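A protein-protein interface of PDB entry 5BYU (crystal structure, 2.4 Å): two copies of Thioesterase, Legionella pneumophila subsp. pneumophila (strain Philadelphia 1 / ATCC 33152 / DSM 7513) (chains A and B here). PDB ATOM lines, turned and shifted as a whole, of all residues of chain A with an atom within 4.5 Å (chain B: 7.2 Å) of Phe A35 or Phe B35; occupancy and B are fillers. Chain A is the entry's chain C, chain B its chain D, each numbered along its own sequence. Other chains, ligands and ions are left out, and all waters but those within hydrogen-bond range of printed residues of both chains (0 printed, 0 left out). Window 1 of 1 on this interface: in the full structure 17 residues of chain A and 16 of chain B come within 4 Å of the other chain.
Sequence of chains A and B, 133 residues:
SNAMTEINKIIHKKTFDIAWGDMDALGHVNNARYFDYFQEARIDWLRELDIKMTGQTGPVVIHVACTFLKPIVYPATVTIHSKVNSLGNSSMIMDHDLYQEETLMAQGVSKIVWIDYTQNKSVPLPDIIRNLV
A ring nitrogen (ND1) of His B63 is in hydrogen-bond range of the backbone carbonyl oxygen (O) of Cys A66, at 3.4 Å.
O of Val B64 is in hydrogen-bond range of N of Cys A66 (2.8 Å).
ND2 of Asn B30 sits at hydrogen-bond distance from OD1 of Asp A36, at 3.2 Å.
The backbone carbonyl oxygen (O) of Val A64 lies within hydrogen-bond range of the backbone NH (N) of Cys B66, at 2.7 Å.
OE1 of Gln A39 sits close to OD1 of Asn B30 (2.8 Å).
The guanidinium group (NH2) of Arg A33 is in salt-bridge range of the side-chain carboxylate (OD2) of Asp B36.
The guanidinium group (NH1) of Arg A33 is in salt-bridge range of the side-chain carboxylate (OD2) of Asp A36.
NH1 of Arg B33 lies within salt-bridge range of OD2 of Asp B36, 3.1 Å away.
The backbone NH (N) of Ala B65 lies within hydrogen-bond range of the backbone carbonyl oxygen (O) of Val B109, at 2.9 Å.
SG of Cys B66 lies close to O of Gln B107 (3.8 Å).
Among the printed residues, pairs that only touch across the chains: Ala A32 with Ala B32 (3.3 Å), Ala A32 with Phe B35 (3.9 Å), Ala A32 with Asp B36 (3.2 Å), Phe A35 with Ala B32 (3.9 Å), Phe A35 with Phe B35 (3.3 Å), Phe A35 with Val B64 (3.5 Å), Asp A36 with Ala B32 (3.2 Å), Val A64 with Phe B35 (3.6 Å), Val A64 with Ala B65 (3.2 Å), Val A64 with Phe B68 (3.6 Å), Ala A65 with His B63 (3.98 Å), Ala A65 with Val B64 (3.2 Å) and Ala A65 with Ala B65 (3.6 Å).
Of the printed residues of chain B, Arg A33 touches Asp B36 (2.5 Å).
Phe A35 touches three residues of chain B.
Printed residues of chain A within 4 Å of Asn B30: Asp A36 (3.2 Å) and Gln A39 (2.8 Å).
Of chain A, only Ala A32 (3.9 Å), Phe A35 (3.3 Å) and Val A64 (3.6 Å) come within 4 Å of Phe B35.
Tyr B37 touches none of the printed residues of chain A.
Of the printed residues of chain A, Ala B65 touches Val A64 (3.2 Å) and Ala A65 (3.6 Å).
Gly B108 touches none of the printed residues of chain A.
Of the 23 printed residues of chain B, 9 touch a printed residue of chain A.
Printed residues of chain B that touch a printed residue of chain A: Asn B30, Ala B32, Phe B35, Asp B36, His B63, Val B64, Ala B65, Cys B66 and Phe B68.
Hydrophobic or aromatic side chains of chain B that line the printed part of chain A: Ala B32, Phe B35, His B63, Val B64, Ala B65 and Phe B68.
Hydrophobic or aromatic side chains of chain A that line the printed part of chain B: Ala A32, Phe A35, Val A64 and Ala A65.
Among the printed residues, Asp or Glu carboxylates within 4 Å of a Lys or Arg side-chain nitrogen of the other chain: Arg A33 with Asp B36.
Ala A32 touches Phe B35, and with the chains exchanged Phe A35 touches Ala B32.
Ala A32 touches Asp B36, and with the chains exchanged Asp A36 touches Ala B32.
Phe B35 touches its own counterpart, Phe A35.
Val A64 touches Ala B65, and with the chains exchanged Ala A65 touches Val B64.
Of the 19 pairs that touch across the chains among the printed residues, 13 have their exchanged pair printed and touching as well.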
ATOM      1  N   ASN A  31       6.589  -8.254 -23.261  1.00  0.00           N
ATOM      2  CA  ASN A  31       6.760  -8.013 -24.693  1.00  0.00           C
ATOM      3  C   ASN A  31       7.266  -9.229 -25.467  1.00  0.00           C
ATOM      4  O   ASN A  31       6.888  -9.432 -26.617  1.00  0.00           O
ATOM      5  CB  ASN A  31       7.694  -6.824 -24.928  1.00  0.00           C
ATOM      6  CG  ASN A  31       7.082  -5.502 -24.496  1.00  0.00           C
ATOM      7  OD1 ASN A  31       5.862  -5.352 -24.454  1.00  0.00           O
ATOM      8  ND2 ASN A  31       7.931  -4.531 -24.184  1.00  0.00           N
ATOM      9  N   ALA A  32       8.121 -10.031 -24.842  1.00  0.00           N
ATOM     10  CA  ALA A  32       8.640 -11.244 -25.477  1.00  0.00           C
ATOM     11  C   ALA A  32       7.527 -12.273 -25.682  1.00  0.00           C
ATOM     12  O   ALA A  32       7.551 -13.089 -26.627  1.00  0.00           O
ATOM     13  CB  ALA A  32       9.761 -11.832 -24.643  1.00  0.00           C
ATOM     14  N   ARG A  33       6.541 -12.214 -24.795  1.00  0.00           N
ATOM     15  CA  ARG A  33       5.429 -13.147 -24.830  1.00  0.00           C
ATOM     16  C   ARG A  33       4.672 -12.968 -26.135  1.00  0.00           C
ATOM     17  O   ARG A  33       4.057 -13.906 -26.637  1.00  0.00           O
ATOM     18  CB  ARG A  33       4.494 -12.935 -23.639  1.00  0.00           C
ATOM     19  CG  ARG A  33       5.155 -13.180 -22.294  1.00  0.00           C
ATOM     20  CD  ARG A  33       5.715 -14.580 -22.182  1.00  0.00           C
ATOM     21  NE  ARG A  33       7.034 -14.549 -21.557  1.00  0.00           N
ATOM     22  CZ  ARG A  33       8.178 -14.668 -22.222  1.00  0.00           C
ATOM     23  NH1 ARG A  33       8.167 -14.834 -23.535  1.00  0.00           N
ATOM     24  NH2 ARG A  33       9.332 -14.625 -21.572  1.00  0.00           N
ATOM     25  N   TYR A  34       4.721 -11.753 -26.678  1.00  0.00           N
ATOM     26  CA  TYR A  34       4.093 -11.464 -27.961  1.00  0.00           C
ATOM     27  C   TYR A  34       4.743 -12.306 -29.050  1.00  0.00           C
ATOM     28  O   TYR A  34       4.062 -12.870 -29.903  1.00  0.00           O
ATOM     29  CB  TYR A  34       4.214  -9.981 -28.330  1.00  0.00           C
ATOM     30  CG  TYR A  34       3.416  -9.022 -27.471  1.00  0.00           C
ATOM     31  CD1 TYR A  34       3.506  -9.053 -26.088  1.00  0.00           C
ATOM     32  CD2 TYR A  34       2.555  -8.101 -28.048  1.00  0.00           C
ATOM     33  CE1 TYR A  34       2.784  -8.180 -25.304  1.00  0.00           C
ATOM     34  CE2 TYR A  34       1.821  -7.226 -27.270  1.00  0.00           C
ATOM     35  CZ  TYR A  34       1.941  -7.272 -25.899  1.00  0.00           C
ATOM     36  OH  TYR A  34       1.216  -6.407 -25.113  1.00  0.00           O
ATOM     37  N   PHE A  35       6.068 -12.390 -29.008  1.00  0.00           N
ATOM     38  CA  PHE A  35       6.801 -13.174 -29.987  1.00  0.00           C
ATOM     39  C   PHE A  35       6.509 -14.649 -29.798  1.00  0.00           C
ATOM     40  O   PHE A  35       6.488 -15.411 -30.768  1.00  0.00           O
ATOM     41  CB  PHE A  35       8.299 -12.889 -29.894  1.00  0.00           C
ATOM     42  CG  PHE A  35       8.662 -11.493 -30.302  1.00  0.00           C
ATOM     43  CD1 PHE A  35       8.732 -11.150 -31.643  1.00  0.00           C
ATOM     44  CD2 PHE A  35       8.907 -10.519 -29.353  1.00  0.00           C
ATOM     45  CE1 PHE A  35       9.054  -9.867 -32.029  1.00  0.00           C
ATOM     46  CE2 PHE A  35       9.231  -9.231 -29.736  1.00  0.00           C
ATOM     47  CZ  PHE A  35       9.303  -8.907 -31.074  1.00  0.00           C
ATOM     48  N   ASP A  36       6.272 -15.056 -28.554  1.00  0.00           N
ATOM     49  CA  ASP A  36       5.772 -16.412 -28.337  1.00  0.00           C
ATOM     50  C   ASP A  36       4.414 -16.615 -29.022  1.00  0.00           C
ATOM     51  O   ASP A  36       4.180 -17.649 -29.657  1.00  0.00           O
ATOM     52  CB  ASP A  36       5.674 -16.729 -26.845  1.00  0.00           C
ATOM     53  CG  ASP A  36       7.027 -17.013 -26.226  1.00  0.00           C
ATOM     54  OD1 ASP A  36       7.857 -17.654 -26.901  1.00  0.00           O
ATOM     55  OD2 ASP A  36       7.259 -16.604 -25.070  1.00  0.00           O
ATOM     56  N   TYR A  37       3.532 -15.623 -28.905  1.00  0.00           N
ATOM     57  CA  TYR A  37       2.208 -15.702 -29.519  1.00  0.00           C
ATOM     58  C   TYR A  37       2.296 -15.838 -31.038  1.00  0.00           C
ATOM     59  O   TYR A  37       1.692 -16.734 -31.631  1.00  0.00           O
ATOM     60  CB  TYR A  37       1.371 -14.459 -29.186  1.00  0.00           C
ATOM     61  CG  TYR A  37       1.080 -14.218 -27.719  1.00  0.00           C
ATOM     62  CD1 TYR A  37       1.124 -15.252 -26.795  1.00  0.00           C
ATOM     63  CD2 TYR A  37       0.755 -12.947 -27.263  1.00  0.00           C
ATOM     64  CE1 TYR A  37       0.850 -15.023 -25.452  1.00  0.00           C
ATOM     65  CE2 TYR A  37       0.484 -12.708 -25.927  1.00  0.00           C
ATOM     66  CZ  TYR A  37       0.533 -13.748 -25.026  1.00  0.00           C
ATOM     67  OH  TYR A  37       0.264 -13.517 -23.697  1.00  0.00           O
ATOM     68  N   PHE A  38       3.054 -14.937 -31.656  1.00  0.00           N
ATOM     69  CA  PHE A  38       3.211 -14.914 -33.104  1.00  0.00           C
ATOM     70  C   PHE A  38       3.861 -16.193 -33.603  1.00  0.00           C
ATOM     71  O   PHE A  38       3.438 -16.761 -34.614  1.00  0.00           O
ATOM     72  CB  PHE A  38       4.035 -13.698 -33.541  1.00  0.00           C
ATOM     73  CG  PHE A  38       3.422 -12.380 -33.163  1.00  0.00           C
ATOM     74  CD1 PHE A  38       2.058 -12.263 -32.969  1.00  0.00           C
ATOM     75  CD2 PHE A  38       4.215 -11.257 -33.003  1.00  0.00           C
ATOM     76  CE1 PHE A  38       1.492 -11.048 -32.622  1.00  0.00           C
ATOM     77  CE2 PHE A  38       3.657 -10.039 -32.655  1.00  0.00           C
ATOM     78  CZ  PHE A  38       2.294  -9.934 -32.465  1.00  0.00           C
ATOM     79  N   GLN A  39       4.906 -16.626 -32.904  1.00  0.00           N
ATOM     80  CA  GLN A  39       5.560 -17.886 -33.216  1.00  0.00           C
ATOM     81  C   GLN A  39       4.536 -19.020 -33.212  1.00  0.00           C
ATOM     82  O   GLN A  39       4.521 -19.853 -34.115  1.00  0.00           O
ATOM     83  CB  GLN A  39       6.703 -18.165 -32.239  1.00  0.00           C
ATOM     84  CG  GLN A  39       7.348 -19.526 -32.420  1.00  0.00           C
ATOM     85  CD  GLN A  39       8.497 -19.762 -31.458  1.00  0.00           C
ATOM     86  OE1 GLN A  39       8.290 -20.129 -30.302  1.00  0.00           O
ATOM     87  NE2 GLN A  39       9.719 -19.558 -31.936  1.00  0.00           N
ATOM     88  N   VAL A  64      12.635 -10.777 -37.071  1.00  0.00           N
ATOM     89  CA  VAL A  64      11.323 -10.623 -36.452  1.00  0.00           C
ATOM     90  C   VAL A  64      11.227  -9.298 -35.691  1.00  0.00           C
ATOM     91  O   VAL A  64      12.206  -8.829 -35.111  1.00  0.00           O
ATOM     92  CB  VAL A  64      11.007 -11.813 -35.515  1.00  0.00           C
ATOM     93  CG1 VAL A  64      11.808 -11.729 -34.227  1.00  0.00           C
ATOM     94  CG2 VAL A  64       9.513 -11.893 -35.236  1.00  0.00           C
ATOM     95  N   ALA A  65      10.043  -8.694 -35.709  1.00  0.00           N
ATOM     96  CA  ALA A  65       9.838  -7.375 -35.122  1.00  0.00           C
ATOM     97  C   ALA A  65       8.410  -7.212 -34.620  1.00  0.00           C
ATOM     98  O   ALA A  65       7.497  -7.879 -35.106  1.00  0.00           O
ATOM     99  CB  ALA A  65      10.169  -6.291 -36.134  1.00  0.00           C
ATOM    100  N   CYS A  66       8.219  -6.320 -33.651  1.00  0.00           N
ATOM    101  CA  CYS A  66       6.884  -6.029 -33.142  1.00  0.00           C
ATOM    102  C   CYS A  66       6.695  -4.555 -32.796  1.00  0.00           C
ATOM    103  O   CYS A  66       7.594  -3.898 -32.277  1.00  0.00           O
ATOM    104  CB  CYS A  66       6.582  -6.887 -31.911  1.00  0.00           C
ATOM    105  SG  CYS A  66       4.853  -6.846 -31.371  1.00  0.00           S
ATOM    106  N   ASN B  30      14.993 -20.453 -28.071  1.00  0.00           N
ATOM    107  CA  ASN B  30      13.756 -20.002 -28.696  1.00  0.00           C
ATOM    108  C   ASN B  30      13.832 -18.500 -28.974  1.00  0.00           C
ATOM    109  O   ASN B  30      14.503 -17.768 -28.244  1.00  0.00           O
ATOM    110  CB  ASN B  30      12.558 -20.340 -27.803  1.00  0.00           C
ATOM    111  CG  ASN B  30      11.232 -20.088 -28.487  1.00  0.00           C
ATOM    112  OD1 ASN B  30      10.870 -20.786 -29.434  1.00  0.00           O
ATOM    113  ND2 ASN B  30      10.493 -19.095 -28.006  1.00  0.00           N
ATOM    114  N   ASN B  31      13.163 -18.040 -30.027  1.00  0.00           N
ATOM    115  CA  ASN B  31      13.334 -16.662 -30.479  1.00  0.00           C
ATOM    116  C   ASN B  31      12.871 -15.573 -29.502  1.00  0.00           C
ATOM    117  O   ASN B  31      13.485 -14.512 -29.442  1.00  0.00           O
ATOM    118  CB  ASN B  31      12.625 -16.456 -31.826  1.00  0.00           C
ATOM    119  CG  ASN B  31      13.281 -17.214 -32.969  1.00  0.00           C
ATOM    120  OD1 ASN B  31      14.468 -17.521 -32.930  1.00  0.00           O
ATOM    121  ND2 ASN B  31      12.504 -17.504 -34.003  1.00  0.00           N
ATOM    122  N   ALA B  32      11.805 -15.823 -28.747  1.00  0.00           N
ATOM    123  CA  ALA B  32      11.305 -14.841 -27.781  1.00  0.00           C
ATOM    124  C   ALA B  32      12.273 -14.606 -26.616  1.00  0.00           C
ATOM    125  O   ALA B  32      12.358 -13.497 -26.051  1.00  0.00           O
ATOM    126  CB  ALA B  32       9.950 -15.281 -27.251  1.00  0.00           C
ATOM    127  N   ARG B  33      13.013 -15.654 -26.264  1.00  0.00           N
ATOM    128  CA  ARG B  33      13.963 -15.578 -25.160  1.00  0.00           C
ATOM    129  C   ARG B  33      15.072 -14.573 -25.431  1.00  0.00           C
ATOM    130  O   ARG B  33      15.655 -14.043 -24.492  1.00  0.00           O
ATOM    131  CB  ARG B  33      14.545 -16.958 -24.840  1.00  0.00           C
ATOM    132  CG  ARG B  33      13.543 -17.904 -24.198  1.00  0.00           C
ATOM    133  CD  ARG B  33      13.073 -17.304 -22.883  1.00  0.00           C
ATOM    134  NE  ARG B  33      14.212 -17.015 -22.013  1.00  0.00           N
ATOM    135  CZ  ARG B  33      14.116 -16.492 -20.796  1.00  0.00           C
ATOM    136  NH1 ARG B  33      12.929 -16.170 -20.300  1.00  0.00           N
ATOM    137  NH2 ARG B  33      15.208 -16.266 -20.080  1.00  0.00           N
ATOM    138  N   TYR B  34      15.383 -14.334 -26.701  1.00  0.00           N
ATOM    139  CA  TYR B  34      16.342 -13.292 -27.046  1.00  0.00           C
ATOM    140  C   TYR B  34      15.829 -11.940 -26.578  1.00  0.00           C
ATOM    141  O   TYR B  34      16.578 -11.125 -26.036  1.00  0.00           O
ATOM    142  CB  TYR B  34      16.599 -13.234 -28.553  1.00  0.00           C
ATOM    143  CG  TYR B  34      17.423 -14.364 -29.118  1.00  0.00           C
ATOM    144  CD1 TYR B  34      16.852 -15.592 -29.419  1.00  0.00           C
ATOM    145  CD2 TYR B  34      18.773 -14.189 -29.378  1.00  0.00           C
ATOM    146  CE1 TYR B  34      17.609 -16.615 -29.948  1.00  0.00           C
ATOM    147  CE2 TYR B  34      19.536 -15.206 -29.906  1.00  0.00           C
ATOM    148  CZ  TYR B  34      18.950 -16.417 -30.190  1.00  0.00           C
ATOM    149  OH  TYR B  34      19.706 -17.438 -30.718  1.00  0.00           O
ATOM    150  N   PHE B  35      14.537 -11.714 -26.786  1.00  0.00           N
ATOM    151  CA  PHE B  35      13.914 -10.469 -26.375  1.00  0.00           C
ATOM    152  C   PHE B  35      13.894 -10.382 -24.859  1.00  0.00           C
ATOM    153  O   PHE B  35      14.059  -9.296 -24.285  1.00  0.00           O
ATOM    154  CB  PHE B  35      12.501 -10.366 -26.956  1.00  0.00           C
ATOM    155  CG  PHE B  35      12.476 -10.219 -28.454  1.00  0.00           C
ATOM    156  CD1 PHE B  35      12.734  -8.993 -29.044  1.00  0.00           C
ATOM    157  CD2 PHE B  35      12.228 -11.311 -29.270  1.00  0.00           C
ATOM    158  CE1 PHE B  35      12.722  -8.851 -30.418  1.00  0.00           C
ATOM    159  CE2 PHE B  35      12.218 -11.173 -30.649  1.00  0.00           C
ATOM    160  CZ  PHE B  35      12.466  -9.942 -31.222  1.00  0.00           C
ATOM    161  N   ASP B  36      13.742 -11.534 -24.209  1.00  0.00           N
ATOM    162  CA  ASP B  36      13.902 -11.586 -22.756  1.00  0.00           C
ATOM    163  C   ASP B  36      15.317 -11.168 -22.330  1.00  0.00           C
ATOM    164  O   ASP B  36      15.482 -10.413 -21.369  1.00  0.00           O
ATOM    165  CB  ASP B  36      13.564 -12.980 -22.227  1.00  0.00           C
ATOM    166  CG  ASP B  36      12.067 -13.241 -22.196  1.00  0.00           C
ATOM    167  OD1 ASP B  36      11.311 -12.306 -21.861  1.00  0.00           O
ATOM    168  OD2 ASP B  36      11.644 -14.372 -22.507  1.00  0.00           O
ATOM    169  N   TYR B  37      16.328 -11.648 -23.049  1.00  0.00           N
ATOM    170  CA  TYR B  37      17.719 -11.308 -22.750  1.00  0.00           C
ATOM    171  C   TYR B  37      17.952  -9.804 -22.875  1.00  0.00           C
ATOM    172  O   TYR B  37      18.499  -9.171 -21.966  1.00  0.00           O
ATOM    173  CB  TYR B  37      18.684 -12.033 -23.692  1.00  0.00           C
ATOM    174  CG  TYR B  37      18.643 -13.546 -23.663  1.00  0.00           C
ATOM    175  CD1 TYR B  37      18.141 -14.239 -22.569  1.00  0.00           C
ATOM    176  CD2 TYR B  37      19.120 -14.280 -24.741  1.00  0.00           C
ATOM    177  CE1 TYR B  37      18.113 -15.625 -22.557  1.00  0.00           C
ATOM    178  CE2 TYR B  37      19.097 -15.661 -24.738  1.00  0.00           C
ATOM    179  CZ  TYR B  37      18.592 -16.328 -23.644  1.00  0.00           C
ATOM    180  OH  TYR B  37      18.565 -17.703 -23.640  1.00  0.00           O
ATOM    181  N   PHE B  38      17.519  -9.242 -24.004  1.00  0.00           N
ATOM    182  CA  PHE B  38      17.721  -7.825 -24.303  1.00  0.00           C
ATOM    183  C   PHE B  38      17.067  -6.957 -23.249  1.00  0.00           C
ATOM    184  O   PHE B  38      17.674  -6.031 -22.697  1.00  0.00           O
ATOM    185  CB  PHE B  38      17.094  -7.465 -25.649  1.00  0.00           C
ATOM    186  CG  PHE B  38      17.610  -8.250 -26.809  1.00  0.00           C
ATOM    187  CD1 PHE B  38      18.881  -8.796 -26.805  1.00  0.00           C
ATOM    188  CD2 PHE B  38      16.793  -8.467 -27.905  1.00  0.00           C
ATOM    189  CE1 PHE B  38      19.334  -9.523 -27.891  1.00  0.00           C
ATOM    190  CE2 PHE B  38      17.235  -9.191 -28.986  1.00  0.00           C
ATOM    191  CZ  PHE B  38      18.507  -9.723 -28.981  1.00  0.00           C
ATOM    192  N   GLN B  39      15.811  -7.294 -22.975  1.00  0.00           N
ATOM    193  CA  GLN B  39      15.023  -6.654 -21.933  1.00  0.00           C
ATOM    194  C   GLN B  39      15.730  -6.699 -20.575  1.00  0.00           C
ATOM    195  O   GLN B  39      15.791  -5.684 -19.873  1.00  0.00           O
ATOM    196  CB  GLN B  39      13.631  -7.298 -21.920  1.00  0.00           C
ATOM    197  CG  GLN B  39      12.690  -7.006 -20.775  1.00  0.00           C
ATOM    198  CD  GLN B  39      11.334  -7.643 -21.041  1.00  0.00           C
ATOM    199  OE1 GLN B  39      10.958  -7.815 -22.200  1.00  0.00           O
ATOM    200  NE2 GLN B  39      10.590  -7.976 -19.984  1.00  0.00           N
ATOM    201  N   GLU B  40      16.282  -7.850 -20.203  1.00  0.00           N
ATOM    202  CA  GLU B  40      16.985  -7.936 -18.923  1.00  0.00           C
ATOM    203  C   GLU B  40      18.257  -7.089 -18.889  1.00  0.00           C
ATOM    204  O   GLU B  40      18.577  -6.491 -17.860  1.00  0.00           O
ATOM    205  CB  GLU B  40      17.327  -9.385 -18.580  1.00  0.00           C
ATOM    206  CG  GLU B  40      16.113 -10.235 -18.272  1.00  0.00           C
ATOM    207  CD  GLU B  40      15.255  -9.626 -17.181  1.00  0.00           C
ATOM    208  OE1 GLU B  40      15.814  -9.064 -16.213  1.00  0.00           O
ATOM    209  OE2 GLU B  40      14.016  -9.700 -17.298  1.00  0.00           O
ATOM    210  N   ALA B  41      18.977  -7.032 -20.006  1.00  0.00           N
ATOM    211  CA  ALA B  41      20.179  -6.200 -20.083  1.00  0.00           C
ATOM    212  C   ALA B  41      19.811  -4.727 -19.882  1.00  0.00           C
ATOM    213  O   ALA B  41      20.458  -3.995 -19.109  1.00  0.00           O
ATOM    214  CB  ALA B  41      20.886  -6.404 -21.415  1.00  0.00           C
ATOM    215  N   ARG B  42      18.753  -4.310 -20.573  1.00  0.00           N
ATOM    216  CA  ARG B  42      18.243  -2.948 -20.463  1.00  0.00           C
ATOM    217  C   ARG B  42      17.886  -2.614 -19.019  1.00  0.00           C
ATOM    218  O   ARG B  42      18.323  -1.589 -18.477  1.00  0.00           O
ATOM    219  CB  ARG B  42      17.015  -2.765 -21.356  1.00  0.00           C
ATOM    220  CG  ARG B  42      16.184  -1.540 -21.014  1.00  0.00           C
ATOM    221  CD  ARG B  42      15.054  -1.321 -22.006  1.00  0.00           C
ATOM    222  NE  ARG B  42      13.979  -2.296 -21.849  1.00  0.00           N
ATOM    223  CZ  ARG B  42      13.706  -3.255 -22.727  1.00  0.00           C
ATOM    224  NH1 ARG B  42      14.428  -3.370 -23.835  1.00  0.00           N
ATOM    225  NH2 ARG B  42      12.707  -4.094 -22.500  1.00  0.00           N
ATOM    226  N   HIS B  63       8.754  -0.146 -30.080  1.00  0.00           N
ATOM    227  CA  HIS B  63       9.126  -1.062 -31.149  1.00  0.00           C
ATOM    228  C   HIS B  63      10.302  -1.921 -30.713  1.00  0.00           C
ATOM    229  O   HIS B  63      11.123  -1.495 -29.914  1.00  0.00           O
ATOM    230  CB  HIS B  63       9.468  -0.288 -32.424  1.00  0.00           C
ATOM    231  CG  HIS B  63       9.693  -1.158 -33.623  1.00  0.00           C
ATOM    232  ND1 HIS B  63       8.669  -1.552 -34.456  1.00  0.00           N
ATOM    233  CD2 HIS B  63      10.822  -1.709 -34.127  1.00  0.00           C
ATOM    234  CE1 HIS B  63       9.158  -2.308 -35.424  1.00  0.00           C
ATOM    235  NE2 HIS B  63      10.461  -2.418 -35.247  1.00  0.00           N
ATOM    236  N   VAL B  64      10.358  -3.148 -31.214  1.00  0.00           N
ATOM    237  CA  VAL B  64      11.503  -4.011 -30.961  1.00  0.00           C
ATOM    238  C   VAL B  64      11.653  -4.991 -32.116  1.00  0.00           C
ATOM    239  O   VAL B  64      10.667  -5.435 -32.707  1.00  0.00           O
ATOM    240  CB  VAL B  64      11.380  -4.758 -29.609  1.00  0.00           C
ATOM    241  CG1 VAL B  64      10.392  -5.897 -29.700  1.00  0.00           C
ATOM    242  CG2 VAL B  64      12.741  -5.266 -29.160  1.00  0.00           C
ATOM    243  N   ALA B  65      12.896  -5.314 -32.443  1.00  0.00           N
ATOM    244  CA  ALA B  65      13.194  -6.146 -33.595  1.00  0.00           C
ATOM    245  C   ALA B  65      14.458  -6.939 -33.339  1.00  0.00           C
ATOM    246  O   ALA B  65      15.305  -6.524 -32.547  1.00  0.00           O
ATOM    247  CB  ALA B  65      13.344  -5.298 -34.846  1.00  0.00           C
ATOM    248  N   CYS B  66      14.587  -8.077 -34.010  1.00  0.00           N
ATOM    249  CA  CYS B  66      15.792  -8.877 -33.887  1.00  0.00           C
ATOM    250  C   CYS B  66      16.189  -9.524 -35.205  1.00  0.00           C
ATOM    251  O   CYS B  66      15.349 -10.004 -35.962  1.00  0.00           O
ATOM    252  CB  CYS B  66      15.608  -9.959 -32.820  1.00  0.00           C
ATOM    253  SG  CYS B  66      17.132 -10.823 -32.378  1.00  0.00           S
ATOM    254  N   THR B  67      17.490  -9.517 -35.460  1.00  0.00           N
ATOM    255  CA  THR B  67      18.075 -10.185 -36.605  1.00  0.00           C
ATOM    256  C   THR B  67      18.879 -11.370 -36.092  1.00  0.00           C
ATOM    257  O   THR B  67      19.746 -11.208 -35.229  1.00  0.00           O
ATOM    258  CB  THR B  67      18.978  -9.237 -37.425  1.00  0.00           C
ATOM    259  OG1 THR B  67      18.223  -8.094 -37.846  1.00  0.00           O
ATOM    260  CG2 THR B  67      19.532  -9.951 -38.647  1.00  0.00           C
ATOM    261  N   PHE B  68      18.570 -12.555 -36.608  1.00  0.00           N
ATOM    262  CA  PHE B  68      19.218 -13.783 -36.163  1.00  0.00           C
ATOM    263  C   PHE B  68      20.294 -14.207 -37.160  1.00  0.00           C
ATOM    264  O   PHE B  68      19.993 -14.600 -38.287  1.00  0.00           O
ATOM    265  CB  PHE B  68      18.188 -14.902 -35.986  1.00  0.00           C
ATOM    266  CG  PHE B  68      16.974 -14.495 -35.191  1.00  0.00           C
ATOM    267  CD1 PHE B  68      17.034 -14.396 -33.811  1.00  0.00           C
ATOM    268  CD2 PHE B  68      15.774 -14.213 -35.827  1.00  0.00           C
ATOM    269  CE1 PHE B  68      15.922 -14.024 -33.077  1.00  0.00           C
ATOM    270  CE2 PHE B  68      14.657 -13.840 -35.098  1.00  0.00           C
ATOM    271  CZ  PHE B  68      14.734 -13.745 -33.722  1.00  0.00           C
ATOM    272  N   HIS B  96      21.100  -3.742 -28.799  1.00  0.00           N
ATOM    273  CA  HIS B  96      21.638  -4.839 -28.014  1.00  0.00           C
ATOM    274  C   HIS B  96      22.285  -5.757 -29.026  1.00  0.00           C
ATOM    275  O   HIS B  96      21.592  -6.379 -29.824  1.00  0.00           O
ATOM    276  CB  HIS B  96      20.561  -5.621 -27.250  1.00  0.00           C
ATOM    277  CG  HIS B  96      19.622  -4.777 -26.444  1.00  0.00           C
ATOM    278  ND1 HIS B  96      19.963  -4.236 -25.226  1.00  0.00           N
ATOM    279  CD2 HIS B  96      18.333  -4.421 -26.669  1.00  0.00           C
ATOM    280  CE1 HIS B  96      18.933  -3.562 -24.742  1.00  0.00           C
ATOM    281  NE2 HIS B  96      17.934  -3.659 -25.598  1.00  0.00           N
ATOM    282  N   GLN B 107      21.169  -9.451 -33.334  1.00  0.00           N
ATOM    283  CA  GLN B 107      21.110  -8.007 -33.133  1.00  0.00           C
ATOM    284  C   GLN B 107      19.698  -7.537 -32.851  1.00  0.00           C
ATOM    285  O   GLN B 107      18.808  -7.703 -33.674  1.00  0.00           O
ATOM    286  CB  GLN B 107      21.647  -7.246 -34.347  1.00  0.00           C
ATOM    287  CG  GLN B 107      23.124  -7.412 -34.621  1.00  0.00           C
ATOM    288  CD  GLN B 107      23.592  -6.513 -35.747  1.00  0.00           C
ATOM    289  OE1 GLN B 107      23.708  -5.297 -35.577  1.00  0.00           O
ATOM    290  NE2 GLN B 107      23.852  -7.101 -36.908  1.00  0.00           N
ATOM    291  N   GLY B 108      19.498  -6.924 -31.696  1.00  0.00           N
ATOM    292  CA  GLY B 108      18.187  -6.421 -31.359  1.00  0.00           C
ATOM    293  C   GLY B 108      18.210  -4.911 -31.383  1.00  0.00           C
ATOM    294  O   GLY B 108      19.169  -4.280 -30.928  1.00  0.00           O
ATOM    295  N   VAL B 109      17.134  -4.334 -31.902  1.00  0.00           N
ATOM    296  CA  VAL B 109      16.978  -2.889 -31.953  1.00  0.00           C
ATOM    297  C   VAL B 109      15.606  -2.538 -31.416  1.00  0.00           C
ATOM    298  O   VAL B 109      14.592  -3.025 -31.915  1.00  0.00           O
ATOM    299  CB  VAL B 109      17.138  -2.330 -33.384  1.00  0.00           C
ATOM    300  CG1 VAL B 109      17.073  -0.814 -33.374  1.00  0.00           C
ATOM    301  CG2 VAL B 109      18.438  -2.809 -34.008  1.00  0.00           C
